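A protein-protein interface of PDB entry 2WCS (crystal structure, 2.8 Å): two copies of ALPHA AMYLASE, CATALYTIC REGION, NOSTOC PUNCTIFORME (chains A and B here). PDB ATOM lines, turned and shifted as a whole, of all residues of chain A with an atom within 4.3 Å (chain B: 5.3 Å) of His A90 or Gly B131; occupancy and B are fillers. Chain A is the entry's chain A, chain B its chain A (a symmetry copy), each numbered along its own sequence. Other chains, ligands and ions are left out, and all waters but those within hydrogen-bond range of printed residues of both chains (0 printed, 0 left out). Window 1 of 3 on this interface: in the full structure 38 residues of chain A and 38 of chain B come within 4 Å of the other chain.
NE2 of His A90 lies within hydrogen-bond range of O of Gly B131, 3.1 Å away.
The backbone carbonyl oxygen (O) of Gly A131 sits at hydrogen-bond distance from a ring nitrogen (NE2) of His B90.
The backbone NH of Gly A131 lies close to a ring nitrogen (ND1) of His B136 (3.2 Å).
A ring nitrogen (ND1) of His A136 lies close to the backbone NH of Gly B131, at 3.2 Å.
His A90 touches just these residues of chain B: Gly B131 (3.1 Å), Phe B133 (3.6 Å) and His B136 (3.9 Å).
Gly B131 touches two residues of chain A.
Of the printed residues of chain A, Tyr B161 touches His A136 (3.96 Å).
Of the printed residues of chain A, Phe B133 touches Gln A80 (3.8 Å), Ser A81 (3.4 Å) and His A90 (3.6 Å).
Printed residues of chain A within 4 Å of Arg B130: His A136 (3.98 Å).
Thr A89 touches none of the printed residues of chain B.
The nearest residue of chain A that does not touch Gly B131 is Gly A131 (4.2 Å).
The nearest printed residue of chain A that does not touch Tyr B161 is Gly A131 (7.4 Å).
Among the printed residues, pairs that only touch across the chains: Gln A80 with Phe B133 (3.8 Å), Ser A81 with Phe B133 (3.4 Å), His A90 with Phe B133 (3.6 Å), His A90 with His B136 (3.9 Å), Ser A129 with His B136 (3.8 Å), Phe A133 with His B90 (3.6 Å), His A136 with His B90 (3.9 Å), His A136 with Ser B129 (3.8 Å), His A136 with Arg B130 (3.98 Å) and His A136 with Tyr B161 (3.96 Å).
His A90 touches Gly B131, and with the chains exchanged Gly A131 touches His B90.
His A90 touches His B136, and with the chains exchanged His A136 touches His B90.
Ser A129 touches His B136, and with the chains exchanged His A136 touches Ser B129.
Gly A131 touches His B136, and with the chains exchanged His A136 touches Gly B131.
Of the 14 pairs that touch across the chains among the printed residues, 10 have their exchanged pair printed and touching as well.
O of Gln A80 lies within hydrogen-bond range of N of His A90 (2.6 Å).
A ring nitrogen (NE2) of His A90 sits at hydrogen-bond distance from the backbone carbonyl oxygen (O) of Gly A131, 3.3 Å away.
OG of Ser A129 lies close to N of Gly A131, at 3.4 Å.
NE2 of His B90 is in hydrogen-bond range of O of Gly B131 (3.3 Å).
OG of Ser B129 sits close to N of Gly B131 (3.4 Å).
The side-chain hydroxyl of Ser B129 lies within hydrogen-bond range of the backbone NH of Phe B132 (3.4 Å).
Along chain B the printed residues that touch a printed residue of chain A span positions 90 to 161.
Among the printed residues, 14 pairs touch across the chains.
Among the printed residues, no Asp or Glu carboxylate lies within 4 Å of a Lys or Arg side-chain nitrogen of the other chain.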
ATOM      1  N   GLN A  80      10.983 -35.488  18.366  1.00  0.00           N
ATOM      2  CA  GLN A  80      10.783 -34.649  19.540  1.00  0.00           C
ATOM      3  C   GLN A  80       9.317 -34.262  19.698  1.00  0.00           C
ATOM      4  O   GLN A  80       8.707 -33.712  18.781  1.00  0.00           O
ATOM      5  CB  GLN A  80      11.652 -33.393  19.456  1.00  0.00           C
ATOM      6  CG  GLN A  80      11.938 -32.744  20.801  1.00  0.00           C
ATOM      7  CD  GLN A  80      12.725 -31.455  20.670  1.00  0.00           C
ATOM      8  OE1 GLN A  80      12.260 -30.488  20.069  1.00  0.00           O
ATOM      9  NE2 GLN A  80      13.927 -31.437  21.234  1.00  0.00           N
ATOM     10  N   SER A  81       8.755 -34.554  20.868  1.00  0.00           N
ATOM     11  CA  SER A  81       7.352 -34.269  21.136  1.00  0.00           C
ATOM     12  C   SER A  81       7.203 -34.225  22.647  1.00  0.00           C
ATOM     13  O   SER A  81       8.108 -34.641  23.363  1.00  0.00           O
ATOM     14  CB  SER A  81       6.470 -35.384  20.575  1.00  0.00           C
ATOM     15  OG  SER A  81       6.838 -36.634  21.136  1.00  0.00           O
ATOM     16  N   HIS A  88       2.316 -35.903  18.656  1.00  0.00           N
ATOM     17  CA  HIS A  88       2.217 -34.452  18.561  1.00  0.00           C
ATOM     18  C   HIS A  88       3.631 -33.965  18.268  1.00  0.00           C
ATOM     19  O   HIS A  88       4.265 -33.328  19.108  1.00  0.00           O
ATOM     20  CB  HIS A  88       1.747 -33.865  19.888  1.00  0.00           C
ATOM     21  CG  HIS A  88       0.393 -34.333  20.319  1.00  0.00           C
ATOM     22  ND1 HIS A  88      -0.769 -33.687  19.960  1.00  0.00           N
ATOM     23  CD2 HIS A  88       0.020 -35.366  21.112  1.00  0.00           C
ATOM     24  CE1 HIS A  88      -1.799 -34.297  20.519  1.00  0.00           C
ATOM     25  NE2 HIS A  88      -1.348 -35.319  21.224  1.00  0.00           N
ATOM     26  N   THR A  89       4.123 -34.279  17.074  1.00  0.00           N
ATOM     27  CA  THR A  89       5.475 -33.906  16.674  1.00  0.00           C
ATOM     28  C   THR A  89       5.785 -32.441  16.914  1.00  0.00           C
ATOM     29  O   THR A  89       5.010 -31.561  16.557  1.00  0.00           O
ATOM     30  CB  THR A  89       5.732 -34.213  15.188  1.00  0.00           C
ATOM     31  OG1 THR A  89       5.320 -35.555  14.892  1.00  0.00           O
ATOM     32  CG2 THR A  89       7.210 -34.071  14.880  1.00  0.00           C
ATOM     33  N   HIS A  90       6.940 -32.195  17.522  1.00  0.00           N
ATOM     34  CA  HIS A  90       7.386 -30.847  17.826  1.00  0.00           C
ATOM     35  C   HIS A  90       8.559 -30.478  16.930  1.00  0.00           C
ATOM     36  O   HIS A  90       8.723 -29.321  16.549  1.00  0.00           O
ATOM     37  CB  HIS A  90       7.787 -30.762  19.300  1.00  0.00           C
ATOM     38  CG  HIS A  90       8.383 -29.446  19.688  1.00  0.00           C
ATOM     39  ND1 HIS A  90       9.708 -29.138  19.469  1.00  0.00           N
ATOM     40  CD2 HIS A  90       7.830 -28.352  20.261  1.00  0.00           C
ATOM     41  CE1 HIS A  90       9.945 -27.909  19.892  1.00  0.00           C
ATOM     42  NE2 HIS A  90       8.822 -27.410  20.375  1.00  0.00           N
ATOM     43  N   ASP A  91       9.368 -31.479  16.600  1.00  0.00           N
ATOM     44  CA  ASP A  91      10.529 -31.300  15.737  1.00  0.00           C
ATOM     45  C   ASP A  91      10.861 -32.623  15.072  1.00  0.00           C
ATOM     46  O   ASP A  91      11.267 -33.575  15.733  1.00  0.00           O
ATOM     47  CB  ASP A  91      11.740 -30.829  16.539  1.00  0.00           C
ATOM     48  CG  ASP A  91      12.960 -30.613  15.667  1.00  0.00           C
ATOM     49  OD1 ASP A  91      14.075 -30.466  16.215  1.00  0.00           O
ATOM     50  OD2 ASP A  91      12.805 -30.584  14.428  1.00  0.00           O
ATOM     51  N   SER A 129       2.047 -30.629  16.048  1.00  0.00           N
ATOM     52  CA  SER A 129       1.645 -30.206  17.380  1.00  0.00           C
ATOM     53  C   SER A 129       1.686 -28.694  17.437  1.00  0.00           C
ATOM     54  O   SER A 129       2.158 -28.052  16.502  1.00  0.00           O
ATOM     55  CB  SER A 129       2.599 -30.766  18.431  1.00  0.00           C
ATOM     56  OG  SER A 129       3.848 -30.107  18.357  1.00  0.00           O
ATOM     57  N   GLY A 131       3.543 -26.898  19.310  1.00  0.00           N
ATOM     58  CA  GLY A 131       4.919 -26.449  19.421  1.00  0.00           C
ATOM     59  C   GLY A 131       5.725 -26.520  18.137  1.00  0.00           C
ATOM     60  O   GLY A 131       6.846 -26.010  18.064  1.00  0.00           O
ATOM     61  N   PHE A 132       5.173 -27.175  17.123  1.00  0.00           N
ATOM     62  CA  PHE A 132       5.867 -27.270  15.852  1.00  0.00           C
ATOM     63  C   PHE A 132       6.151 -25.828  15.445  1.00  0.00           C
ATOM     64  O   PHE A 132       5.238 -25.012  15.338  1.00  0.00           O
ATOM     65  CB  PHE A 132       4.985 -27.963  14.812  1.00  0.00           C
ATOM     66  CG  PHE A 132       5.609 -28.049  13.451  1.00  0.00           C
ATOM     67  CD1 PHE A 132       6.755 -28.811  13.245  1.00  0.00           C
ATOM     68  CD2 PHE A 132       5.065 -27.343  12.380  1.00  0.00           C
ATOM     69  CE1 PHE A 132       7.359 -28.872  11.986  1.00  0.00           C
ATOM     70  CE2 PHE A 132       5.655 -27.394  11.122  1.00  0.00           C
ATOM     71  CZ  PHE A 132       6.810 -28.164  10.923  1.00  0.00           C
ATOM     72  N   PHE A 133       7.424 -25.524  15.234  1.00  0.00           N
ATOM     73  CA  PHE A 133       7.845 -24.175  14.878  1.00  0.00           C
ATOM     74  C   PHE A 133       6.892 -23.325  14.042  1.00  0.00           C
ATOM     75  O   PHE A 133       6.388 -22.310  14.513  1.00  0.00           O
ATOM     76  CB  PHE A 133       9.203 -24.203  14.181  1.00  0.00           C
ATOM     77  CG  PHE A 133       9.641 -22.857  13.694  1.00  0.00           C
ATOM     78  CD1 PHE A 133       9.880 -21.823  14.597  1.00  0.00           C
ATOM     79  CD2 PHE A 133       9.760 -22.599  12.329  1.00  0.00           C
ATOM     80  CE1 PHE A 133      10.225 -20.557  14.151  1.00  0.00           C
ATOM     81  CE2 PHE A 133      10.106 -21.329  11.873  1.00  0.00           C
ATOM     82  CZ  PHE A 133      10.338 -20.308  12.787  1.00  0.00           C
ATOM     83  N   HIS A 136       3.688 -22.547  15.591  1.00  0.00           N
ATOM     84  CA  HIS A 136       4.048 -21.589  16.631  1.00  0.00           C
ATOM     85  C   HIS A 136       4.120 -20.174  16.046  1.00  0.00           C
ATOM     86  O   HIS A 136       3.525 -19.237  16.576  1.00  0.00           O
ATOM     87  CB  HIS A 136       5.410 -21.979  17.211  1.00  0.00           C
ATOM     88  CG  HIS A 136       6.017 -20.944  18.109  1.00  0.00           C
ATOM     89  ND1 HIS A 136       5.746 -20.873  19.458  1.00  0.00           N
ATOM     90  CD2 HIS A 136       6.881 -19.937  17.846  1.00  0.00           C
ATOM     91  CE1 HIS A 136       6.418 -19.867  19.988  1.00  0.00           C
ATOM     92  NE2 HIS A 136       7.114 -19.283  19.031  1.00  0.00           N
ATOM     93  N   HIS B  90      12.954 -19.974  20.261  1.00  0.00           N
ATOM     94  CA  HIS B  90      12.181 -21.191  20.093  1.00  0.00           C
ATOM     95  C   HIS B  90      13.106 -22.399  20.120  1.00  0.00           C
ATOM     96  O   HIS B  90      12.731 -23.472  20.588  1.00  0.00           O
ATOM     97  CB  HIS B  90      11.415 -21.131  18.769  1.00  0.00           C
ATOM     98  CG  HIS B  90      10.683 -22.393  18.437  1.00  0.00           C
ATOM     99  ND1 HIS B  90      11.301 -23.477  17.852  1.00  0.00           N
ATOM    100  CD2 HIS B  90       9.392 -22.750  18.628  1.00  0.00           C
ATOM    101  CE1 HIS B  90      10.419 -24.448  17.696  1.00  0.00           C
ATOM    102  NE2 HIS B  90       9.254 -24.033  18.159  1.00  0.00           N
ATOM    103  N   SER B 129      10.469 -18.594  24.786  1.00  0.00           N
ATOM    104  CA  SER B 129       9.186 -18.342  24.153  1.00  0.00           C
ATOM    105  C   SER B 129       8.263 -19.503  24.460  1.00  0.00           C
ATOM    106  O   SER B 129       8.696 -20.507  25.020  1.00  0.00           O
ATOM    107  CB  SER B 129       9.348 -18.229  22.639  1.00  0.00           C
ATOM    108  OG  SER B 129       9.626 -19.498  22.082  1.00  0.00           O
ATOM    109  N   ARG B 130       6.994 -19.362  24.086  1.00  0.00           N
ATOM    110  CA  ARG B 130       5.998 -20.405  24.310  1.00  0.00           C
ATOM    111  C   ARG B 130       6.334 -21.681  23.529  1.00  0.00           C
ATOM    112  O   ARG B 130       6.038 -22.787  23.980  1.00  0.00           O
ATOM    113  CB  ARG B 130       4.617 -19.908  23.889  1.00  0.00           C
ATOM    114  CG  ARG B 130       4.086 -18.716  24.663  1.00  0.00           C
ATOM    115  CD  ARG B 130       3.697 -17.612  23.699  1.00  0.00           C
ATOM    116  NE  ARG B 130       2.599 -16.794  24.195  1.00  0.00           N
ATOM    117  CZ  ARG B 130       2.123 -15.727  23.563  1.00  0.00           C
ATOM    118  NH1 ARG B 130       2.656 -15.344  22.410  1.00  0.00           N
ATOM    119  NH2 ARG B 130       1.103 -15.048  24.074  1.00  0.00           N
ATOM    120  N   GLY B 131       6.954 -21.518  22.361  1.00  0.00           N
ATOM    121  CA  GLY B 131       7.308 -22.658  21.534  1.00  0.00           C
ATOM    122  C   GLY B 131       8.554 -23.406  21.969  1.00  0.00           C
ATOM    123  O   GLY B 131       8.856 -24.485  21.452  1.00  0.00           O
ATOM    124  N   PHE B 132       9.301 -22.829  22.902  1.00  0.00           N
ATOM    125  CA  PHE B 132      10.496 -23.489  23.391  1.00  0.00           C
ATOM    126  C   PHE B 132      10.027 -24.857  23.875  1.00  0.00           C
ATOM    127  O   PHE B 132       9.144 -24.956  24.724  1.00  0.00           O
ATOM    128  CB  PHE B 132      11.115 -22.691  24.540  1.00  0.00           C
ATOM    129  CG  PHE B 132      12.327 -23.338  25.141  1.00  0.00           C
ATOM    130  CD1 PHE B 132      13.490 -23.499  24.393  1.00  0.00           C
ATOM    131  CD2 PHE B 132      12.296 -23.814  26.451  1.00  0.00           C
ATOM    132  CE1 PHE B 132      14.612 -24.127  24.937  1.00  0.00           C
ATOM    133  CE2 PHE B 132      13.405 -24.442  27.005  1.00  0.00           C
ATOM    134  CZ  PHE B 132      14.572 -24.600  26.243  1.00  0.00           C
ATOM    135  N   PHE B 133      10.616 -25.905  23.316  1.00  0.00           N
ATOM    136  CA  PHE B 133      10.239 -27.272  23.654  1.00  0.00           C
ATOM    137  C   PHE B 133       9.769 -27.553  25.078  1.00  0.00           C
ATOM    138  O   PHE B 133       8.614 -27.905  25.294  1.00  0.00           O
ATOM    139  CB  PHE B 133      11.372 -28.238  23.319  1.00  0.00           C
ATOM    140  CG  PHE B 133      11.087 -29.645  23.744  1.00  0.00           C
ATOM    141  CD1 PHE B 133      10.025 -30.351  23.180  1.00  0.00           C
ATOM    142  CD2 PHE B 133      11.841 -30.252  24.747  1.00  0.00           C
ATOM    143  CE1 PHE B 133       9.717 -31.631  23.612  1.00  0.00           C
ATOM    144  CE2 PHE B 133      11.537 -31.539  25.186  1.00  0.00           C
ATOM    145  CZ  PHE B 133      10.472 -32.227  24.616  1.00  0.00           C
ATOM    146  N   PHE B 135       8.989 -25.663  27.550  1.00  0.00           N
ATOM    147  CA  PHE B 135       7.863 -24.895  28.031  1.00  0.00           C
ATOM    148  C   PHE B 135       6.648 -25.596  27.421  1.00  0.00           C
ATOM    149  O   PHE B 135       5.682 -25.916  28.116  1.00  0.00           O
ATOM    150  CB  PHE B 135       7.940 -23.443  27.554  1.00  0.00           C
ATOM    151  CG  PHE B 135       6.918 -22.552  28.193  1.00  0.00           C
ATOM    152  CD1 PHE B 135       6.868 -22.417  29.582  1.00  0.00           C
ATOM    153  CD2 PHE B 135       5.977 -21.877  27.422  1.00  0.00           C
ATOM    154  CE1 PHE B 135       5.893 -21.626  30.193  1.00  0.00           C
ATOM    155  CE2 PHE B 135       4.999 -21.082  28.021  1.00  0.00           C
ATOM    156  CZ  PHE B 135       4.957 -20.958  29.411  1.00  0.00           C
ATOM    157  N   HIS B 136       6.728 -25.836  26.113  1.00  0.00           N
ATOM    158  CA  HIS B 136       5.686 -26.522  25.355  1.00  0.00           C
ATOM    159  C   HIS B 136       5.237 -27.787  26.096  1.00  0.00           C
ATOM    160  O   HIS B 136       4.046 -28.011  26.305  1.00  0.00           O
ATOM    161  CB  HIS B 136       6.246 -26.900  23.979  1.00  0.00           C
ATOM    162  CG  HIS B 136       5.371 -27.828  23.193  1.00  0.00           C
ATOM    163  ND1 HIS B 136       4.353 -27.384  22.376  1.00  0.00           N
ATOM    164  CD2 HIS B 136       5.364 -29.177  23.101  1.00  0.00           C
ATOM    165  CE1 HIS B 136       3.757 -28.421  21.815  1.00  0.00           C
ATOM    166  NE2 HIS B 136       4.352 -29.520  22.239  1.00  0.00           N
ATOM    167  N   TYR B 161      -1.900 -17.798  25.874  1.00  0.00           N
ATOM    168  CA  TYR B 161      -2.266 -16.970  24.728  1.00  0.00           C
ATOM    169  C   TYR B 161      -3.502 -16.093  24.891  1.00  0.00           C
ATOM    170  O   TYR B 161      -3.556 -14.985  24.349  1.00  0.00           O
ATOM    171  CB  TYR B 161      -2.460 -17.841  23.483  1.00  0.00           C
ATOM    172  CG  TYR B 161      -1.184 -18.354  22.865  1.00  0.00           C
ATOM    173  CD1 TYR B 161      -0.620 -19.563  23.272  1.00  0.00           C
ATOM    174  CD2 TYR B 161      -0.538 -17.629  21.863  1.00  0.00           C
ATOM    175  CE1 TYR B 161       0.553 -20.035  22.695  1.00  0.00           C
ATOM    176  CE2 TYR B 161       0.634 -18.090  21.283  1.00  0.00           C
ATOM    177  CZ  TYR B 161       1.175 -19.292  21.702  1.00  0.00           C
ATOM    178  OH  TYR B 161       2.341 -19.745  21.128  1.00  0.00           O
